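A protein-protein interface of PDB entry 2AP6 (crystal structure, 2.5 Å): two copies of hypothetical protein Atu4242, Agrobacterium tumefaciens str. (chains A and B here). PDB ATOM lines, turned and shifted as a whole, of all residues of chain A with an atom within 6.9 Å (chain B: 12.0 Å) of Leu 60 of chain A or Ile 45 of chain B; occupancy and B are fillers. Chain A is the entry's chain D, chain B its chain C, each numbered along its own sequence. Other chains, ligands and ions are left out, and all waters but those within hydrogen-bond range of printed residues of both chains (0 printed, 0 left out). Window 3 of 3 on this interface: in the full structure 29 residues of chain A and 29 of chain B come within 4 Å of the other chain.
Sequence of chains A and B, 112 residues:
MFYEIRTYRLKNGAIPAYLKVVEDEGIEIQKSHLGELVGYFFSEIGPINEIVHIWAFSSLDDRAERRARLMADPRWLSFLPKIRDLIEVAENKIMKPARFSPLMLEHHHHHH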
ATOM      1  N   PHE A   2     -19.079  -3.589  -6.368  1.00  0.00           N
ATOM      2  CA  PHE A   2     -20.512  -3.755  -6.590  1.00  0.00           C
ATOM      3  C   PHE A   2     -20.785  -3.674  -8.077  1.00  0.00           C
ATOM      4  O   PHE A   2     -20.171  -2.877  -8.782  1.00  0.00           O
ATOM      5  CB  PHE A   2     -21.317  -2.679  -5.868  1.00  0.00           C
ATOM      6  CG  PHE A   2     -21.320  -2.835  -4.380  1.00  0.00           C
ATOM      7  CD1 PHE A   2     -20.346  -2.223  -3.605  1.00  0.00           C
ATOM      8  CD2 PHE A   2     -22.288  -3.622  -3.751  1.00  0.00           C
ATOM      9  CE1 PHE A   2     -20.326  -2.383  -2.224  1.00  0.00           C
ATOM     10  CE2 PHE A   2     -22.276  -3.792  -2.354  1.00  0.00           C
ATOM     11  CZ  PHE A   2     -21.290  -3.168  -1.593  1.00  0.00           C
ATOM     12  N   TYR A   3     -21.691  -4.514  -8.554  1.00  0.00           N
ATOM     13  CA  TYR A   3     -22.038  -4.521  -9.959  1.00  0.00           C
ATOM     14  C   TYR A   3     -23.508  -4.207 -10.132  1.00  0.00           C
ATOM     15  O   TYR A   3     -24.371  -4.878  -9.568  1.00  0.00           O
ATOM     16  CB  TYR A   3     -21.710  -5.877 -10.598  1.00  0.00           C
ATOM     17  CG  TYR A   3     -20.233  -6.144 -10.697  1.00  0.00           C
ATOM     18  CD1 TYR A   3     -19.511  -6.604  -9.596  1.00  0.00           C
ATOM     19  CD2 TYR A   3     -19.535  -5.856 -11.863  1.00  0.00           C
ATOM     20  CE1 TYR A   3     -18.146  -6.759  -9.647  1.00  0.00           C
ATOM     21  CE2 TYR A   3     -18.161  -6.010 -11.925  1.00  0.00           C
ATOM     22  CZ  TYR A   3     -17.479  -6.457 -10.808  1.00  0.00           C
ATOM     23  OH  TYR A   3     -16.118  -6.571 -10.838  1.00  0.00           O
ATOM     24  N   PHE A  57     -19.069  -0.440  -9.103  1.00  0.00           N
ATOM     25  CA  PHE A  57     -18.883   0.625  -8.116  1.00  0.00           C
ATOM     26  C   PHE A  57     -18.144   0.109  -6.881  1.00  0.00           C
ATOM     27  O   PHE A  57     -18.409  -0.989  -6.389  1.00  0.00           O
ATOM     28  CB  PHE A  57     -20.240   1.198  -7.708  1.00  0.00           C
ATOM     29  CG  PHE A  57     -20.945   1.901  -8.814  1.00  0.00           C
ATOM     30  CD1 PHE A  57     -20.548   3.173  -9.206  1.00  0.00           C
ATOM     31  CD2 PHE A  57     -21.980   1.275  -9.506  1.00  0.00           C
ATOM     32  CE1 PHE A  57     -21.174   3.824 -10.282  1.00  0.00           C
ATOM     33  CE2 PHE A  57     -22.611   1.913 -10.581  1.00  0.00           C
ATOM     34  CZ  PHE A  57     -22.207   3.187 -10.969  1.00  0.00           C
ATOM     35  N   SER A  58     -17.218   0.915  -6.374  1.00  0.00           N
ATOM     36  CA  SER A  58     -16.441   0.519  -5.206  1.00  0.00           C
ATOM     37  C   SER A  58     -17.340   0.366  -3.997  1.00  0.00           C
ATOM     38  O   SER A  58     -17.157  -0.553  -3.210  1.00  0.00           O
ATOM     39  CB  SER A  58     -15.348   1.537  -4.923  1.00  0.00           C
ATOM     40  OG  SER A  58     -15.916   2.820  -4.807  1.00  0.00           O
ATOM     41  N   SER A  59     -18.302   1.267  -3.846  1.00  0.00           N
ATOM     42  CA  SER A  59     -19.255   1.192  -2.741  1.00  0.00           C
ATOM     43  C   SER A  59     -20.569   1.760  -3.240  1.00  0.00           C
ATOM     44  O   SER A  59     -20.607   2.436  -4.265  1.00  0.00           O
ATOM     45  CB  SER A  59     -18.767   1.980  -1.528  1.00  0.00           C
ATOM     46  OG  SER A  59     -18.787   3.370  -1.779  1.00  0.00           O
ATOM     47  N   LEU A  60     -21.652   1.474  -2.532  1.00  0.00           N
ATOM     48  CA  LEU A  60     -22.963   1.967  -2.949  1.00  0.00           C
ATOM     49  C   LEU A  60     -23.168   3.463  -2.687  1.00  0.00           C
ATOM     50  O   LEU A  60     -23.985   4.106  -3.343  1.00  0.00           O
ATOM     51  CB  LEU A  60     -24.071   1.131  -2.290  1.00  0.00           C
ATOM     52  CG  LEU A  60     -24.086  -0.319  -2.765  1.00  0.00           C
ATOM     53  CD1 LEU A  60     -25.250  -1.029  -2.132  1.00  0.00           C
ATOM     54  CD2 LEU A  60     -24.176  -0.367  -4.286  1.00  0.00           C
ATOM     55  N   ASP A  61     -22.430   4.013  -1.727  1.00  0.00           N
ATOM     56  CA  ASP A  61     -22.526   5.434  -1.432  1.00  0.00           C
ATOM     57  C   ASP A  61     -21.749   6.180  -2.498  1.00  0.00           C
ATOM     58  O   ASP A  61     -22.044   7.322  -2.813  1.00  0.00           O
ATOM     59  CB  ASP A  61     -21.959   5.736  -0.048  1.00  0.00           C
ATOM     60  CG  ASP A  61     -22.939   5.398   1.057  1.00  0.00           C
ATOM     61  OD1 ASP A  61     -24.126   5.192   0.742  1.00  0.00           O
ATOM     62  OD2 ASP A  61     -22.524   5.350   2.231  1.00  0.00           O
ATOM     63  N   ASP A  62     -20.749   5.509  -3.057  1.00  0.00           N
ATOM     64  CA  ASP A  62     -19.936   6.081  -4.132  1.00  0.00           C
ATOM     65  C   ASP A  62     -20.827   6.082  -5.381  1.00  0.00           C
ATOM     66  O   ASP A  62     -20.815   7.022  -6.172  1.00  0.00           O
ATOM     67  CB  ASP A  62     -18.684   5.211  -4.353  1.00  0.00           C
ATOM     68  CG  ASP A  62     -17.770   5.748  -5.441  1.00  0.00           C
ATOM     69  OD1 ASP A  62     -17.257   6.875  -5.288  1.00  0.00           O
ATOM     70  OD2 ASP A  62     -17.564   5.037  -6.452  1.00  0.00           O
ATOM     71  N   ARG A  63     -21.612   5.018  -5.544  1.00  0.00           N
ATOM     72  CA  ARG A  63     -22.538   4.907  -6.670  1.00  0.00           C
ATOM     73  C   ARG A  63     -23.529   6.064  -6.592  1.00  0.00           C
ATOM     74  O   ARG A  63     -23.774   6.757  -7.570  1.00  0.00           O
ATOM     75  CB  ARG A  63     -23.296   3.566  -6.612  1.00  0.00           C
ATOM     76  CG  ARG A  63     -24.445   3.495  -7.603  1.00  0.00           C
ATOM     77  CD  ARG A  63     -25.122   2.137  -7.649  1.00  0.00           C
ATOM     78  NE  ARG A  63     -26.311   2.191  -8.501  1.00  0.00           N
ATOM     79  CZ  ARG A  63     -27.445   2.810  -8.171  1.00  0.00           C
ATOM     80  NH1 ARG A  63     -27.554   3.423  -6.998  1.00  0.00           N
ATOM     81  NH2 ARG A  63     -28.466   2.842  -9.025  1.00  0.00           N
ATOM     82  N   ALA A  64     -24.092   6.259  -5.409  1.00  0.00           N
ATOM     83  CA  ALA A  64     -25.058   7.320  -5.167  1.00  0.00           C
ATOM     84  C   ALA A  64     -24.459   8.663  -5.527  1.00  0.00           C
ATOM     85  O   ALA A  64     -25.101   9.499  -6.162  1.00  0.00           O
ATOM     86  CB  ALA A  64     -25.469   7.310  -3.705  1.00  0.00           C
ATOM     87  N   GLU A  65     -23.212   8.852  -5.123  1.00  0.00           N
ATOM     88  CA  GLU A  65     -22.475  10.087  -5.353  1.00  0.00           C
ATOM     89  C   GLU A  65     -22.276  10.360  -6.836  1.00  0.00           C
ATOM     90  O   GLU A  65     -22.532  11.463  -7.332  1.00  0.00           O
ATOM     91  CB  GLU A  65     -21.111   9.995  -4.672  1.00  0.00           C
ATOM     92  CG  GLU A  65     -20.779  11.161  -3.786  1.00  0.00           C
ATOM     93  CD  GLU A  65     -19.286  11.298  -3.558  1.00  0.00           C
ATOM     94  OE1 GLU A  65     -18.683  10.330  -3.054  1.00  0.00           O
ATOM     95  OE2 GLU A  65     -18.715  12.370  -3.888  1.00  0.00           O
ATOM     96  N   ASN A  92     -33.176  -2.270 -12.466  1.00  0.00           N
ATOM     97  CA  ASN A  92     -31.755  -2.424 -12.211  1.00  0.00           C
ATOM     98  C   ASN A  92     -31.541  -3.230 -10.940  1.00  0.00           C
ATOM     99  O   ASN A  92     -32.417  -3.287 -10.080  1.00  0.00           O
ATOM    100  CB  ASN A  92     -31.099  -1.041 -12.097  1.00  0.00           C
ATOM    101  CG  ASN A  92     -31.591  -0.245 -10.896  1.00  0.00           C
ATOM    102  OD1 ASN A  92     -32.745  -0.360 -10.490  1.00  0.00           O
ATOM    103  ND2 ASN A  92     -30.716   0.581 -10.337  1.00  0.00           N
ATOM    104  N   LYS A  93     -30.386  -3.874 -10.829  1.00  0.00           N
ATOM    105  CA  LYS A  93     -30.089  -4.668  -9.643  1.00  0.00           C
ATOM    106  C   LYS A  93     -28.614  -4.590  -9.306  1.00  0.00           C
ATOM    107  O   LYS A  93     -27.775  -4.345 -10.177  1.00  0.00           O
ATOM    108  CB  LYS A  93     -30.517  -6.135  -9.838  1.00  0.00           C
ATOM    109  CG  LYS A  93     -29.956  -6.820 -11.076  1.00  0.00           C
ATOM    110  CD  LYS A  93     -30.489  -8.229 -11.206  1.00  0.00           C
ATOM    111  CE  LYS A  93     -30.031  -8.863 -12.511  1.00  0.00           C
ATOM    112  NZ  LYS A  93     -30.592 -10.226 -12.730  1.00  0.00           N
ATOM    113  N   ILE A  94     -28.309  -4.764  -8.024  1.00  0.00           N
ATOM    114  CA  ILE A  94     -26.930  -4.733  -7.547  1.00  0.00           C
ATOM    115  C   ILE A  94     -26.522  -6.147  -7.181  1.00  0.00           C
ATOM    116  O   ILE A  94     -27.262  -6.853  -6.485  1.00  0.00           O
ATOM    117  CB  ILE A  94     -26.775  -3.837  -6.304  1.00  0.00           C
ATOM    118  CG1 ILE A  94     -27.043  -2.382  -6.672  1.00  0.00           C
ATOM    119  CG2 ILE A  94     -25.361  -3.976  -5.738  1.00  0.00           C
ATOM    120  CD1 ILE A  94     -26.116  -1.840  -7.747  1.00  0.00           C
ATOM    121  N   MET A  95     -25.355  -6.566  -7.656  1.00  0.00           N
ATOM    122  CA  MET A  95     -24.869  -7.904  -7.376  1.00  0.00           C
ATOM    123  C   MET A  95     -23.400  -7.848  -6.969  1.00  0.00           C
ATOM    124  O   MET A  95     -22.736  -6.821  -7.112  1.00  0.00           O
ATOM    125  CB  MET A  95     -25.061  -8.808  -8.610  1.00  0.00           C
ATOM    126  CG  MET A  95     -26.512  -8.920  -9.051  1.00  0.00           C
ATOM    127  SD  MET A  95     -26.842 -10.322 -10.328  1.00  0.00           S
ATOM    128  CE  MET A  95     -27.238 -11.788  -9.175  1.00  0.00           C
ATOM    129  N   THR B   7     -29.008 -16.953 -16.001  1.00  0.00           N
ATOM    130  CA  THR B   7     -29.545 -16.499 -14.732  1.00  0.00           C
ATOM    131  C   THR B   7     -30.282 -17.620 -14.027  1.00  0.00           C
ATOM    132  O   THR B   7     -31.224 -18.183 -14.585  1.00  0.00           O
ATOM    133  CB  THR B   7     -30.522 -15.352 -14.951  1.00  0.00           C
ATOM    134  OG1 THR B   7     -29.854 -14.307 -15.661  1.00  0.00           O
ATOM    135  CG2 THR B   7     -31.050 -14.838 -13.626  1.00  0.00           C
ATOM    136  N   ILE B  15     -27.146 -19.989  -2.022  1.00  0.00           N
ATOM    137  CA  ILE B  15     -26.023 -19.313  -2.680  1.00  0.00           C
ATOM    138  C   ILE B  15     -24.647 -19.647  -2.111  1.00  0.00           C
ATOM    139  O   ILE B  15     -23.726 -19.978  -2.866  1.00  0.00           O
ATOM    140  CB  ILE B  15     -26.218 -17.755  -2.701  1.00  0.00           C
ATOM    141  CG1 ILE B  15     -27.207 -17.370  -3.815  1.00  0.00           C
ATOM    142  CG2 ILE B  15     -24.891 -17.045  -2.944  1.00  0.00           C
ATOM    143  CD1 ILE B  15     -27.421 -15.854  -3.969  1.00  0.00           C
ATOM    144  N   PHE B  41     -21.733 -13.360 -10.874  1.00  0.00           N
ATOM    145  CA  PHE B  41     -22.287 -12.612  -9.752  1.00  0.00           C
ATOM    146  C   PHE B  41     -23.419 -13.305  -9.017  1.00  0.00           C
ATOM    147  O   PHE B  41     -24.072 -14.196  -9.546  1.00  0.00           O
ATOM    148  CB  PHE B  41     -22.809 -11.260 -10.240  1.00  0.00           C
ATOM    149  CG  PHE B  41     -21.978 -10.645 -11.318  1.00  0.00           C
ATOM    150  CD1 PHE B  41     -20.770 -10.017 -11.016  1.00  0.00           C
ATOM    151  CD2 PHE B  41     -22.390 -10.711 -12.656  1.00  0.00           C
ATOM    152  CE1 PHE B  41     -19.986  -9.465 -12.025  1.00  0.00           C
ATOM    153  CE2 PHE B  41     -21.610 -10.160 -13.674  1.00  0.00           C
ATOM    154  CZ  PHE B  41     -20.409  -9.536 -13.357  1.00  0.00           C
ATOM    155  N   PHE B  42     -23.634 -12.878  -7.778  1.00  0.00           N
ATOM    156  CA  PHE B  42     -24.724 -13.386  -6.961  1.00  0.00           C
ATOM    157  C   PHE B  42     -25.447 -12.149  -6.429  1.00  0.00           C
ATOM    158  O   PHE B  42     -24.841 -11.092  -6.247  1.00  0.00           O
ATOM    159  CB  PHE B  42     -24.225 -14.294  -5.819  1.00  0.00           C
ATOM    160  CG  PHE B  42     -23.217 -13.655  -4.914  1.00  0.00           C
ATOM    161  CD1 PHE B  42     -21.871 -13.623  -5.262  1.00  0.00           C
ATOM    162  CD2 PHE B  42     -23.605 -13.107  -3.698  1.00  0.00           C
ATOM    163  CE1 PHE B  42     -20.929 -13.057  -4.404  1.00  0.00           C
ATOM    164  CE2 PHE B  42     -22.661 -12.542  -2.843  1.00  0.00           C
ATOM    165  CZ  PHE B  42     -21.324 -12.522  -3.200  1.00  0.00           C
ATOM    166  N   SER B  43     -26.747 -12.281  -6.190  1.00  0.00           N
ATOM    167  CA  SER B  43     -27.562 -11.156  -5.763  1.00  0.00           C
ATOM    168  C   SER B  43     -27.187 -10.445  -4.466  1.00  0.00           C
ATOM    169  O   SER B  43     -26.495 -10.996  -3.606  1.00  0.00           O
ATOM    170  CB  SER B  43     -29.034 -11.580  -5.735  1.00  0.00           C
ATOM    171  OG  SER B  43     -29.232 -12.676  -4.876  1.00  0.00           O
ATOM    172  N   GLU B  44     -27.643  -9.195  -4.369  1.00  0.00           N
ATOM    173  CA  GLU B  44     -27.417  -8.333  -3.215  1.00  0.00           C
ATOM    174  C   GLU B  44     -28.672  -7.478  -3.042  1.00  0.00           C
ATOM    175  O   GLU B  44     -29.278  -7.460  -1.959  1.00  0.00           O
ATOM    176  CB  GLU B  44     -26.182  -7.454  -3.435  1.00  0.00           C
ATOM    177  CG  GLU B  44     -25.906  -6.451  -2.322  1.00  0.00           C
ATOM    178  CD  GLU B  44     -26.065  -7.052  -0.924  1.00  0.00           C
ATOM    179  OE1 GLU B  44     -25.752  -8.261  -0.744  1.00  0.00           O
ATOM    180  OE2 GLU B  44     -26.495  -6.318   0.000  1.00  0.00           O
ATOM    181  N   ILE B  45     -29.054  -6.775  -4.108  1.00  0.00           N
ATOM    182  CA  ILE B  45     -30.264  -5.951  -4.095  1.00  0.00           C
ATOM    183  C   ILE B  45     -31.044  -6.217  -5.376  1.00  0.00           C
ATOM    184  O   ILE B  45     -30.569  -5.948  -6.485  1.00  0.00           O
ATOM    185  CB  ILE B  45     -29.951  -4.443  -3.983  1.00  0.00           C
ATOM    186  CG1 ILE B  45     -29.256  -4.147  -2.649  1.00  0.00           C
ATOM    187  CG2 ILE B  45     -31.241  -3.644  -4.072  1.00  0.00           C
ATOM    188  CD1 ILE B  45     -28.849  -2.711  -2.466  1.00  0.00           C
ATOM    189  N   GLY B  46     -32.241  -6.766  -5.210  1.00  0.00           N
ATOM    190  CA  GLY B  46     -33.095  -7.100  -6.337  1.00  0.00           C
ATOM    191  C   GLY B  46     -33.562  -8.529  -6.143  1.00  0.00           C
ATOM    192  O   GLY B  46     -33.941  -8.883  -5.032  1.00  0.00           O
ATOM    193  N   PRO B  47     -33.566  -9.368  -7.199  1.00  0.00           N
ATOM    194  CA  PRO B  47     -33.999 -10.762  -7.044  1.00  0.00           C
ATOM    195  C   PRO B  47     -33.037 -11.451  -6.065  1.00  0.00           C
ATOM    196  O   PRO B  47     -31.818 -11.374  -6.218  1.00  0.00           O
ATOM    197  CB  PRO B  47     -33.873 -11.313  -8.458  1.00  0.00           C
ATOM    198  CG  PRO B  47     -34.172 -10.113  -9.305  1.00  0.00           C
ATOM    199  CD  PRO B  47     -33.378  -9.033  -8.621  1.00  0.00           C
ATOM    200  N   ILE B  48     -33.596 -12.101  -5.050  1.00  0.00           N
ATOM    201  CA  ILE B  48     -32.800 -12.786  -4.043  1.00  0.00           C
ATOM    202  C   ILE B  48     -32.577 -14.252  -4.436  1.00  0.00           C
ATOM    203  O   ILE B  48     -33.409 -14.848  -5.129  1.00  0.00           O
ATOM    204  CB  ILE B  48     -33.487 -12.662  -2.647  1.00  0.00           C
ATOM    205  CG1 ILE B  48     -33.468 -11.194  -2.193  1.00  0.00           C
ATOM    206  CG2 ILE B  48     -32.766 -13.511  -1.609  1.00  0.00           C
ATOM    207  CD1 ILE B  48     -34.141 -10.951  -0.868  1.00  0.00           C
ATOM    208  N   ASN B  49     -31.442 -14.813  -4.012  1.00  0.00           N
ATOM    209  CA  ASN B  49     -31.065 -16.197  -4.322  1.00  0.00           C
ATOM    210  C   ASN B  49     -30.768 -16.334  -5.816  1.00  0.00           C
ATOM    211  O   ASN B  49     -31.041 -17.368  -6.426  1.00  0.00           O
ATOM    212  CB  ASN B  49     -32.191 -17.169  -3.944  1.00  0.00           C
ATOM    213  CG  ASN B  49     -32.574 -17.068  -2.492  1.00  0.00           C
ATOM    214  OD1 ASN B  49     -31.719 -17.169  -1.600  1.00  0.00           O
ATOM    215  ND2 ASN B  49     -33.862 -16.867  -2.235  1.00  0.00           N
ATOM    216  N   GLU B  50     -30.193 -15.290  -6.403  1.00  0.00           N
ATOM    217  CA  GLU B  50     -29.904 -15.314  -7.824  1.00  0.00           C
ATOM    218  C   GLU B  50     -28.437 -15.358  -8.194  1.00  0.00           C
ATOM    219  O   GLU B  50     -27.600 -14.753  -7.553  1.00  0.00           O
ATOM    220  CB  GLU B  50     -30.548 -14.105  -8.497  1.00  0.00           C
ATOM    221  CG  GLU B  50     -30.546 -14.169  -9.997  1.00  0.00           C
ATOM    222  CD  GLU B  50     -31.093 -12.920 -10.620  1.00  0.00           C
ATOM    223  OE1 GLU B  50     -30.417 -11.881 -10.529  1.00  0.00           O
ATOM    224  OE2 GLU B  50     -32.199 -12.979 -11.198  1.00  0.00           O
ATOM    225  N   ILE B  51     -28.156 -16.090  -9.262  1.00  0.00           N
ATOM    226  CA  ILE B  51     -26.812 -16.229  -9.805  1.00  0.00           C
ATOM    227  C   ILE B  51     -26.866 -15.797 -11.272  1.00  0.00           C
ATOM    228  O   ILE B  51     -27.765 -16.179 -12.021  1.00  0.00           O
ATOM    229  CB  ILE B  51     -26.303 -17.701  -9.756  1.00  0.00           C
ATOM    230  CG1 ILE B  51     -26.111 -18.159  -8.306  1.00  0.00           C
ATOM    231  CG2 ILE B  51     -25.020 -17.828 -10.563  1.00  0.00           C
ATOM    232  CD1 ILE B  51     -25.010 -17.431  -7.538  1.00  0.00           C
ATOM    233  N   VAL B  52     -25.896 -14.983 -11.663  1.00  0.00           N
ATOM    234  CA  VAL B  52     -25.787 -14.499 -13.023  1.00  0.00           C
ATOM    235  C   VAL B  52     -24.334 -14.601 -13.465  1.00  0.00           C
ATOM    236  O   VAL B  52     -23.453 -14.009 -12.845  1.00  0.00           O
ATOM    237  CB  VAL B  52     -26.222 -13.022 -13.131  1.00  0.00           C
ATOM    238  CG1 VAL B  52     -25.782 -12.431 -14.470  1.00  0.00           C
ATOM    239  CG2 VAL B  52     -27.723 -12.916 -12.968  1.00  0.00           C
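Of the printed residues of chain B, Leu 60 of chain A touches Ile 45 (3.99 Å). Of the printed residues of chain A, Ile 45 of chain B touches Leu 60, Lys 93 and Ile 94. No residue of chain B comes within 4 Å of Phe 2 of chain A. No residue of chain B comes within 4 Å of Ser 58 of chain A. No residue of chain B comes within 4 Å of Asp 61 of chain A. No residue of chain B comes within 4 Å of Arg 63 of chain A. Printed residues of chain B within 4 Å of Lys 93 of chain A: Ile 45 (3.4 Å), Pro 47 (3.96 Å), Glu 50 (2.8 Å) and Val 52 (3.9 Å). Of chain B, only Glu 44 (3.2 Å) and Ile 45 (3.0 Å) come within 4 Å of Ile 94 of chain A. Met 95 of chain A touches five residues of chain B. Of the printed residues of chain B, Tyr 3 of chain A touches Phe 41. Of the printed residues of chain A, Val 52 of chain B touches Lys 93 and Met 95. Glu 65 of chain A touches none of the printed residues of chain B. The nearest printed residue of chain B that does not touch Leu 60 of chain A is Glu 44 of chain B (5.5 Å). The nearest printed residue of chain A that does not touch Ile 45 of chain B is Asn 92 of chain A (4.8 Å). The nearest printed residue of chain A that does not touch Phe 41 of chain B is Phe 2 of chain A (7.0 Å).
The backbone carbonyl oxygen (O) of Ile 94 of chain A sits at hydrogen-bond distance from the backbone NH (N) of Glu 44 of chain B (3.2 Å). The backbone NH (N) of Ile 45 of chain B is in hydrogen-bond range of the backbone carbonyl oxygen (O) of Ile 94 of chain A, at 3.0 Å. The side-chain carboxylate of Glu 50 of chain B lies within salt-bridge range of the side-chain amino group of Lys 93 of chain A, 2.8 Å away.
Tyr 3 of chain A touches Phe 41 of chain B. Ile 45 of chain B touches Leu 60 of chain A. Lys 93 of chain A touches Ile 45 of chain B (CB to O, 3.4 Å). Pro 47 of chain B touches Lys 93 of chain A (CD to CD, 3.96 Å). CG2 of Val 52 of chain B touches NZ of Lys 93 of chain A (3.9 Å). Phe 41 of chain B touches Met 95 of chain A (CB to CB, 3.7 Å). CB of Met 95 of chain A touches O of Phe 42 of chain B, at 3.3 Å. Ser 43 of chain B touches Met 95 of chain A. O of Glu 50 of chain B touches CE of Met 95 of chain A, 3.4 Å away. SD of Met 95 of chain A touches CG2 of Val 52 of chain B, at 3.8 Å.
The backbone NH of Phe 41 of chain B sits at hydrogen-bond distance from the backbone carbonyl oxygen of Val 52 of chain B (2.7 Å). OG of Ser 43 of chain B sits close to O of Pro 47 of chain B. The backbone NH of Asn 49 of chain B lies within hydrogen-bond range of the side-chain hydroxyl of Ser 43 of chain B, 3.2 Å away. The backbone NH of Ser 43 of chain B lies within hydrogen-bond range of the backbone carbonyl oxygen of Glu 50 of chain B. The backbone NH (N) of Met 95 of chain A lies within hydrogen-bond range of the backbone carbonyl oxygen (O) of Tyr 3 of chain A (2.7 Å).
Of the 14 printed residues of chain B, 8 touch a printed residue of chain A. Printed residues of chain B that touch a printed residue of chain A: Phe 41, Phe 42, Ser 43, Glu 44, Ile 45, Pro 47, Glu 50 and Val 52. Hydrophobic or aromatic side chains of chain B that line the printed part of chain A: Phe 41, Ile 45, Pro 47 and Val 52. Of the 15 printed residues of chain A, 5 touch a printed residue of chain B. Printed residues of chain A that touch a printed residue of chain B: Tyr 3, Leu 60, Lys 93, Ile 94 and Met 95.
No position is printed for both chains. Of the 13 pairs that touch across the chains among the printed residues, none has its exchanged pair printed and touching as well.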
